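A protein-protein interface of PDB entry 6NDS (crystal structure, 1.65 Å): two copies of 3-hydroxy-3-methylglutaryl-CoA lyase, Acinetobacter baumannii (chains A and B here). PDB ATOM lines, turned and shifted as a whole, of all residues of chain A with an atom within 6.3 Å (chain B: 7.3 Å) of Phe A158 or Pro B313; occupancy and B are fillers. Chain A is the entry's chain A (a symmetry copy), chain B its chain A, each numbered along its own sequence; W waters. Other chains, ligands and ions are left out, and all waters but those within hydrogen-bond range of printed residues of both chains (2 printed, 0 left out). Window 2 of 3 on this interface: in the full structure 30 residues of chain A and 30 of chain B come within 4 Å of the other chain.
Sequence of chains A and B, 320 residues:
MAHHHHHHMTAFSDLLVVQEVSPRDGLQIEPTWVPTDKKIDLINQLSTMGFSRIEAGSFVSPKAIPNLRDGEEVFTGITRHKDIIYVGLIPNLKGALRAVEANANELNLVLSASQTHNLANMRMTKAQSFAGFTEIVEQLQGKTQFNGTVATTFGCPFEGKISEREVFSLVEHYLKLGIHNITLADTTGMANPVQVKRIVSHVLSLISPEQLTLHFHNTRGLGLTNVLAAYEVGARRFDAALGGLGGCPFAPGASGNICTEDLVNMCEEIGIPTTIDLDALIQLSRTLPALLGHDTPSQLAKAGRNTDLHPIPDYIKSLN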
ATOM      1  N   SER A 114     -26.525  -4.127   7.225  1.00  0.00           N
ATOM      2  CA  SER A 114     -25.952  -3.289   6.185  1.00  0.00           C
ATOM      3  C   SER A 114     -26.427  -1.855   6.381  1.00  0.00           C
ATOM      4  O   SER A 114     -27.637  -1.604   6.378  1.00  0.00           O
ATOM      5  CB  SER A 114     -26.382  -3.796   4.812  1.00  0.00           C
ATOM      6  OG  SER A 114     -26.246  -2.775   3.835  1.00  0.00           O
ATOM      7  N   THR A 116     -26.144   0.497   4.222  1.00  0.00           N
ATOM      8  CA  THR A 116     -26.791   0.916   2.980  1.00  0.00           C
ATOM      9  C   THR A 116     -28.226   0.415   2.916  1.00  0.00           C
ATOM     10  O   THR A 116     -29.144   1.157   2.542  1.00  0.00           O
ATOM     11  CB  THR A 116     -26.013   0.405   1.767  1.00  0.00           C
ATOM     12  OG1 THR A 116     -24.674   0.908   1.796  1.00  0.00           O
ATOM     13  CG2 THR A 116     -26.701   0.850   0.484  1.00  0.00           C
ATOM     14  N   HIS A 117     -28.444  -0.855   3.268  1.00  0.00           N
ATOM     15  CA  HIS A 117     -29.798  -1.388   3.246  1.00  0.00           C
ATOM     16  C   HIS A 117     -30.677  -0.737   4.312  1.00  0.00           C
ATOM     17  O   HIS A 117     -31.866  -0.501   4.075  1.00  0.00           O
ATOM     18  CB  HIS A 117     -29.766  -2.907   3.422  1.00  0.00           C
ATOM     19  CG  HIS A 117     -31.089  -3.564   3.205  1.00  0.00           C
ATOM     20  ND1 HIS A 117     -31.946  -3.868   4.240  1.00  0.00           N
ATOM     21  CD2 HIS A 117     -31.705  -3.974   2.071  1.00  0.00           C
ATOM     22  CE1 HIS A 117     -33.037  -4.433   3.753  1.00  0.00           C
ATOM     23  NE2 HIS A 117     -32.913  -4.514   2.441  1.00  0.00           N
ATOM     24  N   ALA A 120     -31.729   2.492   2.868  1.00  0.00           N
ATOM     25  CA  ALA A 120     -32.679   2.322   1.770  1.00  0.00           C
ATOM     26  C   ALA A 120     -34.062   1.920   2.271  1.00  0.00           C
ATOM     27  O   ALA A 120     -35.074   2.325   1.689  1.00  0.00           O
ATOM     28  CB  ALA A 120     -32.167   1.271   0.785  1.00  0.00           C
ATOM     29  N   CYS A 156     -25.717  -8.601   1.777  1.00  0.00           N
ATOM     30  CA  CYS A 156     -26.538  -7.469   1.386  1.00  0.00           C
ATOM     31  C   CYS A 156     -26.546  -7.321  -0.129  1.00  0.00           C
ATOM     32  O   CYS A 156     -25.496  -7.443  -0.772  1.00  0.00           O
ATOM     33  CB  CYS A 156     -25.995  -6.189   2.030  1.00  0.00           C
ATOM     34  SG  CYS A 156     -26.748  -4.660   1.427  1.00  0.00           S
ATOM     35  N   PRO A 157     -27.714  -7.062  -0.730  1.00  0.00           N
ATOM     36  CA  PRO A 157     -27.761  -6.877  -2.190  1.00  0.00           C
ATOM     37  C   PRO A 157     -27.034  -5.627  -2.671  1.00  0.00           C
ATOM     38  O   PRO A 157     -26.749  -5.517  -3.872  1.00  0.00           O
ATOM     39  CB  PRO A 157     -29.267  -6.789  -2.486  1.00  0.00           C
ATOM     40  CG  PRO A 157     -29.860  -6.257  -1.200  1.00  0.00           C
ATOM     41  CD  PRO A 157     -29.037  -6.892  -0.099  1.00  0.00           C
ATOM     42  N   PHE A 158     -26.741  -4.673  -1.781  1.00  0.00           N
ATOM     43  CA  PHE A 158     -25.989  -3.477  -2.140  1.00  0.00           C
ATOM     44  C   PHE A 158     -24.508  -3.601  -1.816  1.00  0.00           C
ATOM     45  O   PHE A 158     -23.656  -3.292  -2.654  1.00  0.00           O
ATOM     46  CB  PHE A 158     -26.542  -2.245  -1.411  1.00  0.00           C
ATOM     47  CG  PHE A 158     -27.980  -1.953  -1.700  1.00  0.00           C
ATOM     48  CD1 PHE A 158     -28.369  -1.500  -2.951  1.00  0.00           C
ATOM     49  CD2 PHE A 158     -28.940  -2.088  -0.705  1.00  0.00           C
ATOM     50  CE1 PHE A 158     -29.698  -1.201  -3.218  1.00  0.00           C
ATOM     51  CE2 PHE A 158     -30.279  -1.796  -0.964  1.00  0.00           C
ATOM     52  CZ  PHE A 158     -30.652  -1.349  -2.221  1.00  0.00           C
ATOM     53  N   GLU A 159     -24.191  -4.032  -0.593  1.00  0.00           N
ATOM     54  CA  GLU A 159     -22.824  -4.020  -0.092  1.00  0.00           C
ATOM     55  C   GLU A 159     -22.093  -5.334  -0.328  1.00  0.00           C
ATOM     56  O   GLU A 159     -20.855  -5.348  -0.337  1.00  0.00           O
ATOM     57  CB  GLU A 159     -22.821  -3.693   1.410  1.00  0.00           C
ATOM     58  CG  GLU A 159     -23.348  -2.285   1.733  1.00  0.00           C
ATOM     59  CD  GLU A 159     -23.167  -1.885   3.197  1.00  0.00           C
ATOM     60  OE1 GLU A 159     -22.668  -2.713   3.992  1.00  0.00           O
ATOM     61  OE2 GLU A 159     -23.528  -0.737   3.552  1.00  0.00           O
ATOM     62  N   GLY A 160     -22.816  -6.416  -0.536  1.00  0.00           N
ATOM     63  CA  GLY A 160     -22.192  -7.726  -0.704  1.00  0.00           C
ATOM     64  C   GLY A 160     -21.966  -8.405   0.643  1.00  0.00           C
ATOM     65  O   GLY A 160     -22.924  -8.630   1.389  1.00  0.00           O
ATOM     66  N   PHE A 250     -37.718  -2.921  -1.047  1.00  0.00           N
ATOM     67  CA  PHE A 250     -36.553  -2.046  -1.031  1.00  0.00           C
ATOM     68  C   PHE A 250     -35.235  -2.812  -1.010  1.00  0.00           C
ATOM     69  O   PHE A 250     -34.169  -2.190  -0.976  1.00  0.00           O
ATOM     70  CB  PHE A 250     -36.647  -1.084   0.160  1.00  0.00           C
ATOM     71  CG  PHE A 250     -37.885  -0.231   0.135  1.00  0.00           C
ATOM     72  CD1 PHE A 250     -38.003   0.809  -0.775  1.00  0.00           C
ATOM     73  CD2 PHE A 250     -38.943  -0.483   0.996  1.00  0.00           C
ATOM     74  CE1 PHE A 250     -39.146   1.592  -0.817  1.00  0.00           C
ATOM     75  CE2 PHE A 250     -40.092   0.302   0.956  1.00  0.00           C
ATOM     76  CZ  PHE A 250     -40.191   1.334   0.049  1.00  0.00           C
ATOM     77  N   ALA A 251     -35.286  -4.147  -1.040  1.00  0.00           N
ATOM     78  CA  ALA A 251     -34.105  -4.959  -1.285  1.00  0.00           C
ATOM     79  C   ALA A 251     -34.165  -5.454  -2.724  1.00  0.00           C
ATOM     80  O   ALA A 251     -34.978  -6.341  -3.028  1.00  0.00           O
ATOM     81  CB  ALA A 251     -34.044  -6.133  -0.308  1.00  0.00           C
ATOM     82  N   PRO A 252     -33.347  -4.920  -3.637  1.00  0.00           N
ATOM     83  CA  PRO A 252     -33.553  -5.191  -5.067  1.00  0.00           C
ATOM     84  C   PRO A 252     -33.430  -6.674  -5.385  1.00  0.00           C
ATOM     85  O   PRO A 252     -32.528  -7.361  -4.900  1.00  0.00           O
ATOM     86  CB  PRO A 252     -32.441  -4.381  -5.748  1.00  0.00           C
ATOM     87  CG  PRO A 252     -31.975  -3.404  -4.718  1.00  0.00           C
ATOM     88  CD  PRO A 252     -32.158  -4.090  -3.401  1.00  0.00           C
ATOM     89  N   ASP B 308     -23.564 -10.375  -7.956  1.00  0.00           N
ATOM     90  CA  ASP B 308     -24.285  -9.429  -8.811  1.00  0.00           C
ATOM     91  C   ASP B 308     -24.970  -8.415  -7.904  1.00  0.00           C
ATOM     92  O   ASP B 308     -26.104  -8.608  -7.466  1.00  0.00           O
ATOM     93  CB  ASP B 308     -25.290 -10.156  -9.697  1.00  0.00           C
ATOM     94  CG  ASP B 308     -24.636 -10.880 -10.847  1.00  0.00           C
ATOM     95  OD1 ASP B 308     -23.400 -10.761 -11.010  1.00  0.00           O
ATOM     96  OD2 ASP B 308     -25.359 -11.562 -11.603  1.00  0.00           O
ATOM     97  N   LEU B 309     -24.270  -7.325  -7.606  1.00  0.00           N
ATOM     98  CA  LEU B 309     -24.779  -6.331  -6.677  1.00  0.00           C
ATOM     99  C   LEU B 309     -25.668  -5.326  -7.407  1.00  0.00           C
ATOM    100  O   LEU B 309     -25.650  -5.207  -8.634  1.00  0.00           O
ATOM    101  CB  LEU B 309     -23.630  -5.611  -5.960  1.00  0.00           C
ATOM    102  CG  LEU B 309     -22.690  -6.536  -5.177  1.00  0.00           C
ATOM    103  CD1 LEU B 309     -21.600  -5.721  -4.489  1.00  0.00           C
ATOM    104  CD2 LEU B 309     -23.461  -7.382  -4.165  1.00  0.00           C
ATOM    105  N   HIS B 310     -26.456  -4.598  -6.630  1.00  0.00           N
ATOM    106  CA  HIS B 310     -27.425  -3.681  -7.202  1.00  0.00           C
ATOM    107  C   HIS B 310     -27.055  -2.241  -6.875  1.00  0.00           C
ATOM    108  O   HIS B 310     -26.455  -1.970  -5.828  1.00  0.00           O
ATOM    109  CB  HIS B 310     -28.835  -3.998  -6.684  1.00  0.00           C
ATOM    110  CG  HIS B 310     -29.282  -5.395  -6.986  1.00  0.00           C
ATOM    111  ND1 HIS B 310     -30.182  -5.690  -7.986  1.00  0.00           N
ATOM    112  CD2 HIS B 310     -28.937  -6.580  -6.428  1.00  0.00           C
ATOM    113  CE1 HIS B 310     -30.381  -6.996  -8.024  1.00  0.00           C
ATOM    114  NE2 HIS B 310     -29.633  -7.559  -7.093  1.00  0.00           N
ATOM    115  N   PRO B 311     -27.381  -1.299  -7.756  1.00  0.00           N
ATOM    116  CA  PRO B 311     -26.965   0.088  -7.532  1.00  0.00           C
ATOM    117  C   PRO B 311     -27.697   0.707  -6.353  1.00  0.00           C
ATOM    118  O   PRO B 311     -28.862   0.402  -6.085  1.00  0.00           O
ATOM    119  CB  PRO B 311     -27.333   0.785  -8.847  1.00  0.00           C
ATOM    120  CG  PRO B 311     -28.461  -0.035  -9.397  1.00  0.00           C
ATOM    121  CD  PRO B 311     -28.161  -1.456  -8.999  1.00  0.00           C
ATOM    122  N   ILE B 312     -26.992   1.578  -5.645  1.00  0.00           N
ATOM    123  CA  ILE B 312     -27.580   2.257  -4.484  1.00  0.00           C
ATOM    124  C   ILE B 312     -28.555   3.326  -4.970  1.00  0.00           C
ATOM    125  O   ILE B 312     -28.196   4.132  -5.849  1.00  0.00           O
ATOM    126  CB  ILE B 312     -26.482   2.867  -3.611  1.00  0.00           C
ATOM    127  N   PRO B 313     -29.788   3.380  -4.441  1.00  0.00           N
ATOM    128  CA  PRO B 313     -30.840   4.307  -4.885  1.00  0.00           C
ATOM    129  C   PRO B 313     -30.436   5.781  -4.821  1.00  0.00           C
ATOM    130  O   PRO B 313     -29.477   6.130  -4.133  1.00  0.00           O
ATOM    131  CB  PRO B 313     -31.988   4.026  -3.908  1.00  0.00           C
ATOM    132  CG  PRO B 313     -31.751   2.639  -3.435  1.00  0.00           C
ATOM    133  CD  PRO B 313     -30.261   2.488  -3.368  1.00  0.00           C
HETATM  134  O   HOH W   1     -31.148  -9.694  -5.028  1.00  0.00           O
HETATM  135  O   HOH W   2     -23.944  -1.699  -4.924  1.00  0.00           O
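The side-chain hydroxyl (OG) of Ser A114 is in hydrogen-bond range of the side-chain sulfur (SG) of Cys A156 (3.1 Å).
SG of Cys A156 sits close to N of Phe A158 (3.2 Å).
The side-chain sulfur (SG) of Cys A156 sits at hydrogen-bond distance from the backbone NH (N) of Glu A159.
N of His B310 sits at hydrogen-bond distance from O of Pro A157 (2.9 Å).
Phe A158 touches just these residues of chain B: Leu B309, His B310, Pro B311 and Pro B313.
Of the printed residues of chain A, Pro B313 touches Phe A158 (3.7 Å).
Printed residues of chain B within 4 Å of Pro A157: Leu B309 and His B310.
Of the printed residues of chain A, His B310 touches Pro A157, Phe A158 and Pro A252.
Printed residues of chain B within 4 Å of Pro A252: His B310.
Printed residues of chain A within 4 Å of Pro B311: Phe A158.
Of the printed residues of chain B, Gly A160 touches Leu B309 (3.7 Å).
Asp B308 touches none of the printed residues of chain A.
Ala A251 touches none of the printed residues of chain B.
The nearest residue of chain B that does not touch Phe A158 is Ile B312 (4.1 Å).
The nearest printed residue of chain A that does not touch His B310 is Glu A159 (6.1 Å).
Hydrophobic or aromatic side chains of chain B within 4 Å of the printed part of chain A: Leu B309, His B310 and Pro B313.
Hydrophobic or aromatic side chains of chain A that line the printed part of chain B: Pro A157, Phe A158 and Pro A252.
Among the printed residues, no Asp or Glu carboxylate lies within 4 Å of a Lys or Arg side-chain nitrogen of the other chain.
Water W2 lies within hydrogen-bond range of the backbone carbonyl oxygen (O) of His B310 and the backbone carbonyl oxygen (O) of Phe A158.
Water W1 lies within hydrogen-bond range of the backbone carbonyl oxygen (O) of Pro A252 and a ring nitrogen (NE2) of His B310.
Cys A156 touches Leu B309 (O to CD2, 3.96 Å).
O of Pro A157 touches CA of Leu B309, 3.5 Å away.
Leu B309 touches Phe A158 (CD1 to O, 3.7 Å).
CD1 of Phe A158 touches O of His B310, 3.5 Å away.
Pro B311 touches Phe A158.
Pro B313 touches Phe A158.
CA of Gly A160 touches CD2 of Leu B309 (3.7 Å).
CB of Pro A252 touches ND1 of His B310 (3.4 Å).
No position is printed for both chains.
Of the 9 pairs that touch across the chains among the printed residues, none has its exchanged pair printed and touching as well.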
